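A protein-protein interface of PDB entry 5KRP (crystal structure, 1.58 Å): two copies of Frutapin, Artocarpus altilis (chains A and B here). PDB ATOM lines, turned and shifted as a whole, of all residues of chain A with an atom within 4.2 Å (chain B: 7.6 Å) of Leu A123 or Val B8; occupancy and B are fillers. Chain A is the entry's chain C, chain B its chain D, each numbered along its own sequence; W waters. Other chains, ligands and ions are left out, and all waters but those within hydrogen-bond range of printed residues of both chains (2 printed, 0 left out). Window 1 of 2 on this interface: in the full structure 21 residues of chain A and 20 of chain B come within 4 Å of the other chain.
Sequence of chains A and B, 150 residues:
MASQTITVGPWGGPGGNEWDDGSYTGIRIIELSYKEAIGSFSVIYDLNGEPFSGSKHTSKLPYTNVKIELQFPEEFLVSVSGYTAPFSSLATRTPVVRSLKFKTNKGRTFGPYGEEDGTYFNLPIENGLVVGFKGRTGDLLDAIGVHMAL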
ATOM      1  N   VAL A   8     -25.646  15.099  -5.427  1.00  0.00           N
ATOM      2  CA  VAL A   8     -25.082  15.077  -6.761  1.00  0.00           C
ATOM      3  C   VAL A   8     -26.125  15.451  -7.813  1.00  0.00           C
ATOM      4  O   VAL A   8     -27.327  15.364  -7.564  1.00  0.00           O
ATOM      5  CB  VAL A   8     -24.491  13.726  -7.053  1.00  0.00           C
ATOM      6  CG1 VAL A   8     -23.331  13.504  -6.134  1.00  0.00           C
ATOM      7  CG2 VAL A   8     -25.417  12.566  -6.955  1.00  0.00           C
ATOM      8  N   VAL A  78     -30.234   1.079  -7.059  1.00  0.00           N
ATOM      9  CA  VAL A  78     -28.795   1.036  -7.290  1.00  0.00           C
ATOM     10  C   VAL A  78     -28.315   1.832  -8.550  1.00  0.00           C
ATOM     11  O   VAL A  78     -27.096   1.818  -8.922  1.00  0.00           O
ATOM     12  CB  VAL A  78     -28.299  -0.409  -7.369  1.00  0.00           C
ATOM     13  CG1 VAL A  78     -28.612  -1.179  -6.099  1.00  0.00           C
ATOM     14  CG2 VAL A  78     -28.841  -1.179  -8.566  1.00  0.00           C
ATOM     15  N   SER A  79     -29.250   2.407  -9.325  1.00  0.00           N
ATOM     16  CA  SER A  79     -28.919   3.157 -10.527  1.00  0.00           C
ATOM     17  C   SER A  79     -30.047   4.155 -10.808  1.00  0.00           C
ATOM     18  O   SER A  79     -31.212   3.790 -10.740  1.00  0.00           O
ATOM     19  CB  SER A  79     -28.734   2.248 -11.774  1.00  0.00           C
ATOM     20  OG  SER A  79     -28.500   3.003 -12.952  1.00  0.00           O
ATOM     21  N   VAL A  80     -29.657   5.405 -11.089  1.00  0.00           N
ATOM     22  CA  VAL A  80     -30.519   6.393 -11.694  1.00  0.00           C
ATOM     23  C   VAL A  80     -29.875   6.842 -13.003  1.00  0.00           C
ATOM     24  O   VAL A  80     -28.734   7.189 -13.024  1.00  0.00           O
ATOM     25  CB  VAL A  80     -30.772   7.608 -10.790  1.00  0.00           C
ATOM     26  CG1 VAL A  80     -31.654   8.617 -11.464  1.00  0.00           C
ATOM     27  CG2 VAL A  80     -31.359   7.153  -9.490  1.00  0.00           C
ATOM     28  N   ASN A 122     -25.799   8.936 -16.037  1.00  0.00           N
ATOM     29  CA  ASN A 122     -25.886   7.649 -15.394  1.00  0.00           C
ATOM     30  C   ASN A 122     -25.193   7.743 -14.042  1.00  0.00           C
ATOM     31  O   ASN A 122     -23.994   8.134 -13.979  1.00  0.00           O
ATOM     32  CB  ASN A 122     -25.091   6.717 -16.259  1.00  0.00           C
ATOM     33  CG  ASN A 122     -24.946   5.379 -15.685  1.00  0.00           C
ATOM     34  OD1 ASN A 122     -25.825   4.908 -14.982  1.00  0.00           O
ATOM     35  ND2 ASN A 122     -23.813   4.731 -15.989  1.00  0.00           N
ATOM     36  N   LEU A 123     -25.915   7.387 -12.983  1.00  0.00           N
ATOM     37  CA  LEU A 123     -25.419   7.339 -11.595  1.00  0.00           C
ATOM     38  C   LEU A 123     -25.550   5.918 -11.036  1.00  0.00           C
ATOM     39  O   LEU A 123     -26.543   5.545 -10.395  1.00  0.00           O
ATOM     40  CB  LEU A 123     -26.149   8.287 -10.667  1.00  0.00           C
ATOM     41  CG  LEU A 123     -25.548   8.387  -9.240  1.00  0.00           C
ATOM     42  CD1 LEU A 123     -24.234   9.131  -9.183  1.00  0.00           C
ATOM     43  CD2 LEU A 123     -26.585   9.064  -8.364  1.00  0.00           C
ATOM     44  N   PRO A 124     -24.504   5.107 -11.241  1.00  0.00           N
ATOM     45  CA  PRO A 124     -24.450   3.838 -10.577  1.00  0.00           C
ATOM     46  C   PRO A 124     -24.061   4.003  -9.137  1.00  0.00           C
ATOM     47  O   PRO A 124     -23.117   4.781  -8.831  1.00  0.00           O
ATOM     48  CB  PRO A 124     -23.286   3.083 -11.337  1.00  0.00           C
ATOM     49  CG  PRO A 124     -22.928   3.948 -12.464  1.00  0.00           C
ATOM     50  CD  PRO A 124     -23.312   5.349 -12.099  1.00  0.00           C
ATOM     51  N   ILE A 125     -24.753   3.288  -8.241  1.00  0.00           N
ATOM     52  CA  ILE A 125     -24.467   3.357  -6.796  1.00  0.00           C
ATOM     53  C   ILE A 125     -23.901   1.995  -6.361  1.00  0.00           C
ATOM     54  O   ILE A 125     -24.616   0.984  -6.344  1.00  0.00           O
ATOM     55  CB  ILE A 125     -25.717   3.666  -5.976  1.00  0.00           C
ATOM     56  CG1 ILE A 125     -26.411   4.944  -6.561  1.00  0.00           C
ATOM     57  CG2 ILE A 125     -25.355   3.843  -4.499  1.00  0.00           C
ATOM     58  CD1 ILE A 125     -27.771   5.215  -5.925  1.00  0.00           C
ATOM     59  N   VAL A 146     -29.935  13.984  -6.800  1.00  0.00           N
ATOM     60  CA  VAL A 146     -30.192  13.036  -5.713  1.00  0.00           C
ATOM     61  C   VAL A 146     -29.392  13.389  -4.448  1.00  0.00           C
ATOM     62  O   VAL A 146     -28.239  13.797  -4.545  1.00  0.00           O
ATOM     63  CB  VAL A 146     -30.003  11.548  -6.012  1.00  0.00           C
ATOM     64  CG1 VAL A 146     -31.005  11.108  -7.067  1.00  0.00           C
ATOM     65  CG2 VAL A 146     -28.677  11.299  -6.510  1.00  0.00           C
ATOM     66  N   MET A 148     -27.856  11.574  -1.092  1.00  0.00           N
ATOM     67  CA  MET A 148     -27.445  10.208  -0.731  1.00  0.00           C
ATOM     68  C   MET A 148     -26.976  10.134   0.696  1.00  0.00           C
ATOM     69  O   MET A 148     -26.381  11.100   1.233  1.00  0.00           O
ATOM     70  CB  MET A 148     -26.331   9.762  -1.668  1.00  0.00           C
ATOM     71  CG  MET A 148     -26.706   9.842  -3.151  1.00  0.00           C
ATOM     72  SD  MET A 148     -25.423   9.179  -4.176  1.00  0.00           S
ATOM     73  CE  MET A 148     -25.655   7.449  -3.787  1.00  0.00           C
ATOM     74  N   THR B   5     -17.907   4.794   3.107  1.00  0.00           N
ATOM     75  CA  THR B   5     -18.289   5.996   2.366  1.00  0.00           C
ATOM     76  C   THR B   5     -19.248   5.606   1.237  1.00  0.00           C
ATOM     77  O   THR B   5     -19.188   4.494   0.699  1.00  0.00           O
ATOM     78  CB  THR B   5     -17.062   6.709   1.739  1.00  0.00           C
ATOM     79  OG1 THR B   5     -16.304   5.782   0.993  1.00  0.00           O
ATOM     80  CG2 THR B   5     -16.157   7.260   2.818  1.00  0.00           C
ATOM     81  N   ILE B   6     -20.032   6.584   0.826  1.00  0.00           N
ATOM     82  CA  ILE B   6     -20.850   6.504  -0.397  1.00  0.00           C
ATOM     83  C   ILE B   6     -19.906   6.269  -1.578  1.00  0.00           C
ATOM     84  O   ILE B   6     -18.834   6.946  -1.657  1.00  0.00           O
ATOM     85  CB  ILE B   6     -21.578   7.816  -0.670  1.00  0.00           C
ATOM     86  CG1 ILE B   6     -22.550   8.197   0.463  1.00  0.00           C
ATOM     87  CG2 ILE B   6     -22.298   7.708  -1.996  1.00  0.00           C
ATOM     88  CD1 ILE B   6     -23.439   7.119   0.857  1.00  0.00           C
ATOM     89  N   THR B   7     -20.246   5.310  -2.448  1.00  0.00           N
ATOM     90  CA  THR B   7     -19.416   4.981  -3.610  1.00  0.00           C
ATOM     91  C   THR B   7     -20.307   4.967  -4.843  1.00  0.00           C
ATOM     92  O   THR B   7     -21.305   4.227  -4.904  1.00  0.00           O
ATOM     93  CB  THR B   7     -18.708   3.633  -3.425  1.00  0.00           C
ATOM     94  OG1 THR B   7     -17.977   3.674  -2.208  1.00  0.00           O
ATOM     95  CG2 THR B   7     -17.725   3.406  -4.549  1.00  0.00           C
ATOM     96  N   VAL B   8     -19.962   5.813  -5.783  1.00  0.00           N
ATOM     97  CA  VAL B   8     -20.657   5.931  -7.063  1.00  0.00           C
ATOM     98  C   VAL B   8     -19.756   5.583  -8.229  1.00  0.00           C
ATOM     99  O   VAL B   8     -18.526   5.550  -8.130  1.00  0.00           O
ATOM    100  CB  VAL B   8     -21.320   7.260  -7.293  1.00  0.00           C
ATOM    101  CG1 VAL B   8     -22.437   7.459  -6.300  1.00  0.00           C
ATOM    102  CG2 VAL B   8     -20.304   8.366  -7.165  1.00  0.00           C
ATOM    103  N   GLY B   9     -20.391   5.217  -9.350  1.00  0.00           N
ATOM    104  CA  GLY B   9     -19.668   4.516 -10.441  1.00  0.00           C
ATOM    105  C   GLY B   9     -19.535   3.042 -10.141  1.00  0.00           C
ATOM    106  O   GLY B   9     -20.284   2.521  -9.341  1.00  0.00           O
ATOM    107  N   PRO B  10     -18.597   2.345 -10.763  1.00  0.00           N
ATOM    108  CA  PRO B  10     -17.725   2.908 -11.792  1.00  0.00           C
ATOM    109  C   PRO B  10     -18.368   3.214 -13.130  1.00  0.00           C
ATOM    110  O   PRO B  10     -19.531   2.744 -13.435  1.00  0.00           O
ATOM    111  CB  PRO B  10     -16.658   1.828 -12.003  1.00  0.00           C
ATOM    112  CG  PRO B  10     -16.930   0.762 -11.021  1.00  0.00           C
ATOM    113  CD  PRO B  10     -18.315   0.942 -10.501  1.00  0.00           C
ATOM    114  N   TRP B  11     -17.645   4.051 -13.881  1.00  0.00           N
ATOM    115  CA  TRP B  11     -17.932   4.355 -15.293  1.00  0.00           C
ATOM    116  C   TRP B  11     -16.828   3.692 -16.114  1.00  0.00           C
ATOM    117  O   TRP B  11     -15.622   3.932 -15.834  1.00  0.00           O
ATOM    118  CB  TRP B  11     -17.980   5.821 -15.465  1.00  0.00           C
ATOM    119  CG  TRP B  11     -19.183   6.453 -14.786  1.00  0.00           C
ATOM    120  CD1 TRP B  11     -20.478   6.527 -15.276  1.00  0.00           C
ATOM    121  CD2 TRP B  11     -19.216   7.109 -13.499  1.00  0.00           C
ATOM    122  NE1 TRP B  11     -21.309   7.235 -14.364  1.00  0.00           N
ATOM    123  CE2 TRP B  11     -20.550   7.594 -13.283  1.00  0.00           C
ATOM    124  CE3 TRP B  11     -18.235   7.368 -12.518  1.00  0.00           C
ATOM    125  CZ2 TRP B  11     -20.922   8.274 -12.114  1.00  0.00           C
ATOM    126  CZ3 TRP B  11     -18.608   8.050 -11.360  1.00  0.00           C
ATOM    127  CH2 TRP B  11     -19.959   8.467 -11.166  1.00  0.00           C
ATOM    128  N   ASN B 122     -20.855  12.056 -16.255  1.00  0.00           N
ATOM    129  CA  ASN B 122     -20.661  13.340 -15.594  1.00  0.00           C
ATOM    130  C   ASN B 122     -21.229  13.255 -14.180  1.00  0.00           C
ATOM    131  O   ASN B 122     -22.409  12.836 -14.023  1.00  0.00           O
ATOM    132  CB  ASN B 122     -21.391  14.335 -16.438  1.00  0.00           C
ATOM    133  CG  ASN B 122     -21.545  15.605 -15.804  1.00  0.00           C
ATOM    134  OD1 ASN B 122     -20.598  16.107 -15.194  1.00  0.00           O
ATOM    135  ND2 ASN B 122     -22.760  16.193 -15.929  1.00  0.00           N
ATOM    136  N   LEU B 123     -20.392  13.621 -13.196  1.00  0.00           N
ATOM    137  CA  LEU B 123     -20.780  13.629 -11.737  1.00  0.00           C
ATOM    138  C   LEU B 123     -20.603  15.005 -11.260  1.00  0.00           C
ATOM    139  O   LEU B 123     -19.506  15.403 -10.807  1.00  0.00           O
ATOM    140  CB  LEU B 123     -19.981  12.629 -10.912  1.00  0.00           C
ATOM    141  CG  LEU B 123     -20.269  12.517  -9.393  1.00  0.00           C
ATOM    142  CD1 LEU B 123     -21.619  11.896  -9.288  1.00  0.00           C
ATOM    143  CD2 LEU B 123     -19.193  11.686  -8.667  1.00  0.00           C
ATOM    144  N   PRO B 124     -21.668  15.788 -11.319  1.00  0.00           N
ATOM    145  CA  PRO B 124     -21.634  17.094 -10.674  1.00  0.00           C
ATOM    146  C   PRO B 124     -21.927  16.935  -9.174  1.00  0.00           C
ATOM    147  O   PRO B 124     -22.798  16.094  -8.794  1.00  0.00           O
ATOM    148  CB  PRO B 124     -22.766  17.879 -11.324  1.00  0.00           C
ATOM    149  CG  PRO B 124     -23.400  16.966 -12.286  1.00  0.00           C
ATOM    150  CD  PRO B 124     -22.933  15.578 -12.044  1.00  0.00           C
ATOM    151  N   ILE B 125     -21.130  17.642  -8.354  1.00  0.00           N
ATOM    152  CA  ILE B 125     -21.252  17.505  -6.907  1.00  0.00           C
ATOM    153  C   ILE B 125     -21.747  18.806  -6.360  1.00  0.00           C
ATOM    154  O   ILE B 125     -21.064  19.803  -6.451  1.00  0.00           O
ATOM    155  CB  ILE B 125     -19.920  17.124  -6.208  1.00  0.00           C
ATOM    156  CG1 ILE B 125     -19.391  15.797  -6.756  1.00  0.00           C
ATOM    157  CG2 ILE B 125     -20.190  16.997  -4.717  1.00  0.00           C
ATOM    158  CD1 ILE B 125     -17.912  15.612  -6.495  1.00  0.00           C
ATOM    159  N   GLY B 132     -11.833   9.592  -2.294  1.00  0.00           N
ATOM    160  CA  GLY B 132     -11.156   8.384  -2.785  1.00  0.00           C
ATOM    161  C   GLY B 132     -11.537   7.973  -4.153  1.00  0.00           C
ATOM    162  O   GLY B 132     -12.618   8.312  -4.592  1.00  0.00           O
ATOM    163  N   LYS B 134     -11.637   4.462  -6.935  1.00  0.00           N
ATOM    164  CA  LYS B 134     -11.463   3.042  -7.217  1.00  0.00           C
ATOM    165  C   LYS B 134     -11.585   2.838  -8.743  1.00  0.00           C
ATOM    166  O   LYS B 134     -12.012   3.733  -9.446  1.00  0.00           O
ATOM    167  CB  LYS B 134     -12.479   2.188  -6.504  1.00  0.00           C
ATOM    168  CG  LYS B 134     -13.897   2.386  -6.915  1.00  0.00           C
ATOM    169  CD  LYS B 134     -14.855   1.606  -6.033  1.00  0.00           C
ATOM    170  CE  LYS B 134     -14.674   0.113  -5.850  1.00  0.00           C
ATOM    171  NZ  LYS B 134     -15.168  -0.699  -6.956  1.00  0.00           N
ATOM    172  N   ILE B 144     -13.482   3.752 -13.711  1.00  0.00           N
ATOM    173  CA  ILE B 144     -13.158   4.670 -12.626  1.00  0.00           C
ATOM    174  C   ILE B 144     -14.444   4.975 -11.852  1.00  0.00           C
ATOM    175  O   ILE B 144     -15.513   5.103 -12.445  1.00  0.00           O
ATOM    176  CB  ILE B 144     -12.490   5.958 -13.142  1.00  0.00           C
ATOM    177  CG1 ILE B 144     -11.917   6.722 -11.960  1.00  0.00           C
ATOM    178  CG2 ILE B 144     -13.434   6.805 -14.019  1.00  0.00           C
ATOM    179  CD1 ILE B 144     -11.049   7.879 -12.239  1.00  0.00           C
ATOM    180  N   GLY B 145     -14.332   4.988 -10.510  1.00  0.00           N
ATOM    181  CA  GLY B 145     -15.414   5.347  -9.592  1.00  0.00           C
ATOM    182  C   GLY B 145     -14.885   6.113  -8.408  1.00  0.00           C
ATOM    183  O   GLY B 145     -13.686   6.358  -8.303  1.00  0.00           O
ATOM    184  N   VAL B 146     -15.786   6.710  -7.626  1.00  0.00           N
ATOM    185  CA  VAL B 146     -15.397   7.674  -6.629  1.00  0.00           C
ATOM    186  C   VAL B 146     -16.105   7.403  -5.301  1.00  0.00           C
ATOM    187  O   VAL B 146     -17.286   7.017  -5.268  1.00  0.00           O
ATOM    188  CB  VAL B 146     -15.671   9.159  -7.017  1.00  0.00           C
ATOM    189  CG1 VAL B 146     -15.127   9.456  -8.438  1.00  0.00           C
ATOM    190  CG2 VAL B 146     -17.106   9.500  -6.967  1.00  0.00           C
ATOM    191  N   HIS B 147     -15.349   7.628  -4.235  1.00  0.00           N
ATOM    192  CA  HIS B 147     -15.836   7.641  -2.863  1.00  0.00           C
ATOM    193  C   HIS B 147     -16.080   9.071  -2.460  1.00  0.00           C
ATOM    194  O   HIS B 147     -15.247   9.945  -2.708  1.00  0.00           O
ATOM    195  CB  HIS B 147     -14.828   7.058  -1.886  1.00  0.00           C
ATOM    196  CG  HIS B 147     -14.493   5.636  -2.125  1.00  0.00           C
ATOM    197  ND1 HIS B 147     -15.431   4.636  -2.060  1.00  0.00           N
ATOM    198  CD2 HIS B 147     -13.307   5.030  -2.427  1.00  0.00           C
ATOM    199  CE1 HIS B 147     -14.857   3.464  -2.280  1.00  0.00           C
ATOM    200  NE2 HIS B 147     -13.576   3.681  -2.535  1.00  0.00           N
ATOM    201  N   MET B 148     -17.229   9.287  -1.771  1.00  0.00           N
ATOM    202  CA  MET B 148     -17.635  10.606  -1.322  1.00  0.00           C
ATOM    203  C   MET B 148     -17.942  10.679   0.160  1.00  0.00           C
ATOM    204  O   MET B 148     -18.443   9.714   0.738  1.00  0.00           O
ATOM    205  CB  MET B 148     -18.865  11.161  -2.120  1.00  0.00           C
ATOM    206  CG  MET B 148     -18.591  11.152  -3.631  1.00  0.00           C
ATOM    207  SD  MET B 148     -20.081  11.686  -4.533  1.00  0.00           S
ATOM    208  CE  MET B 148     -19.764  13.385  -4.270  1.00  0.00           C
HETATM  209  O   HOH W   1     -23.320  10.433 -15.840  1.00  0.00           O
HETATM  210  O   HOH W   2     -21.561   2.986 -15.476  1.00  0.00           O
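O of Pro A124 sits at hydrogen-bond distance from N of Gly B9, at 2.8 Å.
The indole nitrogen of Trp B11 lies within hydrogen-bond range of the backbone carbonyl oxygen of Asn A122, 2.9 Å away.
Among the printed residues, pairs that only touch across the chains: Val A8 with Pro B124 (3.2 Å), Pro A124 with Val B8 (3.2 Å), Pro A124 with Trp B11 (3.6 Å), Ile A125 with Thr B7 (3.7 Å), Pro A124 with Pro B10 (3.7 Å), Leu A123 with Val B8 (3.8 Å), Leu A123 with Leu B123 (3.8 Å), Met A148 with Ile B6 (3.8 Å) and Val A8 with Leu B123 (3.9 Å).
Water W2 lies within hydrogen-bond range of O of Pro B10 (2.9 Å) and ND2 of Asn A122 (2.9 Å).
Water W1 lies within hydrogen-bond range of the backbone NH of Asn A122 (2.9 Å) and the backbone NH of Asn B122 (3.0 Å).
Hydrophobic or aromatic side chains of chain A that line the printed part of chain B: Val A8, Leu A123, Pro A124 and Met A148.
Of the 18 printed residues of chain B, 8 touch a printed residue of chain A.
Printed residues of chain B that touch a printed residue of chain A: Ile B6, Thr B7, Val B8, Gly B9, Pro B10, Trp B11, Leu B123 and Pro B124.
Hydrophobic or aromatic side chains of chain B within 4 Å of the printed part of chain A: Ile B6, Val B8, Trp B11 and Leu B123.
Among the printed residues, no Asp or Glu carboxylate lies within 4 Å of a Lys or Arg side-chain nitrogen of the other chain.
O of Thr B5 is in hydrogen-bond range of OG1 of Thr B7 (3.3 Å).
N of Trp B11 is in hydrogen-bond range of O of Ile B144 (2.8 Å).
The backbone carbonyl oxygen (O) of Ile B6 lies within hydrogen-bond range of the backbone NH (N) of Met B148, 2.8 Å away.
O of Val B146 lies within hydrogen-bond range of N of Val B8.
The backbone NH (N) of Ile A125 sits at hydrogen-bond distance from the backbone carbonyl oxygen (O) of Val A78 (2.8 Å).
The backbone NH of Val A8 sits at hydrogen-bond distance from the backbone carbonyl oxygen of Val A146, at 3.0 Å.
Printed residues of chain B within 4 Å of Val A8: Leu B123 and Pro B124.
Printed residues of chain B within 4 Å of Leu A123: Val B8 (3.8 Å) and Leu B123 (3.8 Å).
Of the printed residues of chain B, Ile A125 touches Thr B7 (3.7 Å).
Printed residues of chain B within 4 Å of Met A148: Ile B6.
Val B8 touches just these residues of chain A: Leu A123 and Pro A124.
Of the printed residues of chain A, Gly B9 touches Pro A124 (2.8 Å).
Of the printed residues of chain A, Leu B123 touches Val A8 and Leu A123.
Val A8 touches Leu B123, and with the chains exchanged Leu A123 touches Val B8.
Val A8 touches Pro B124, and with the chains exchanged Pro A124 touches Val B8.
Leu A123 touches its own counterpart, Leu B123.
Of the 11 pairs that touch across the chains among the printed residues, 5 have their exchanged pair printed and touching as well.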
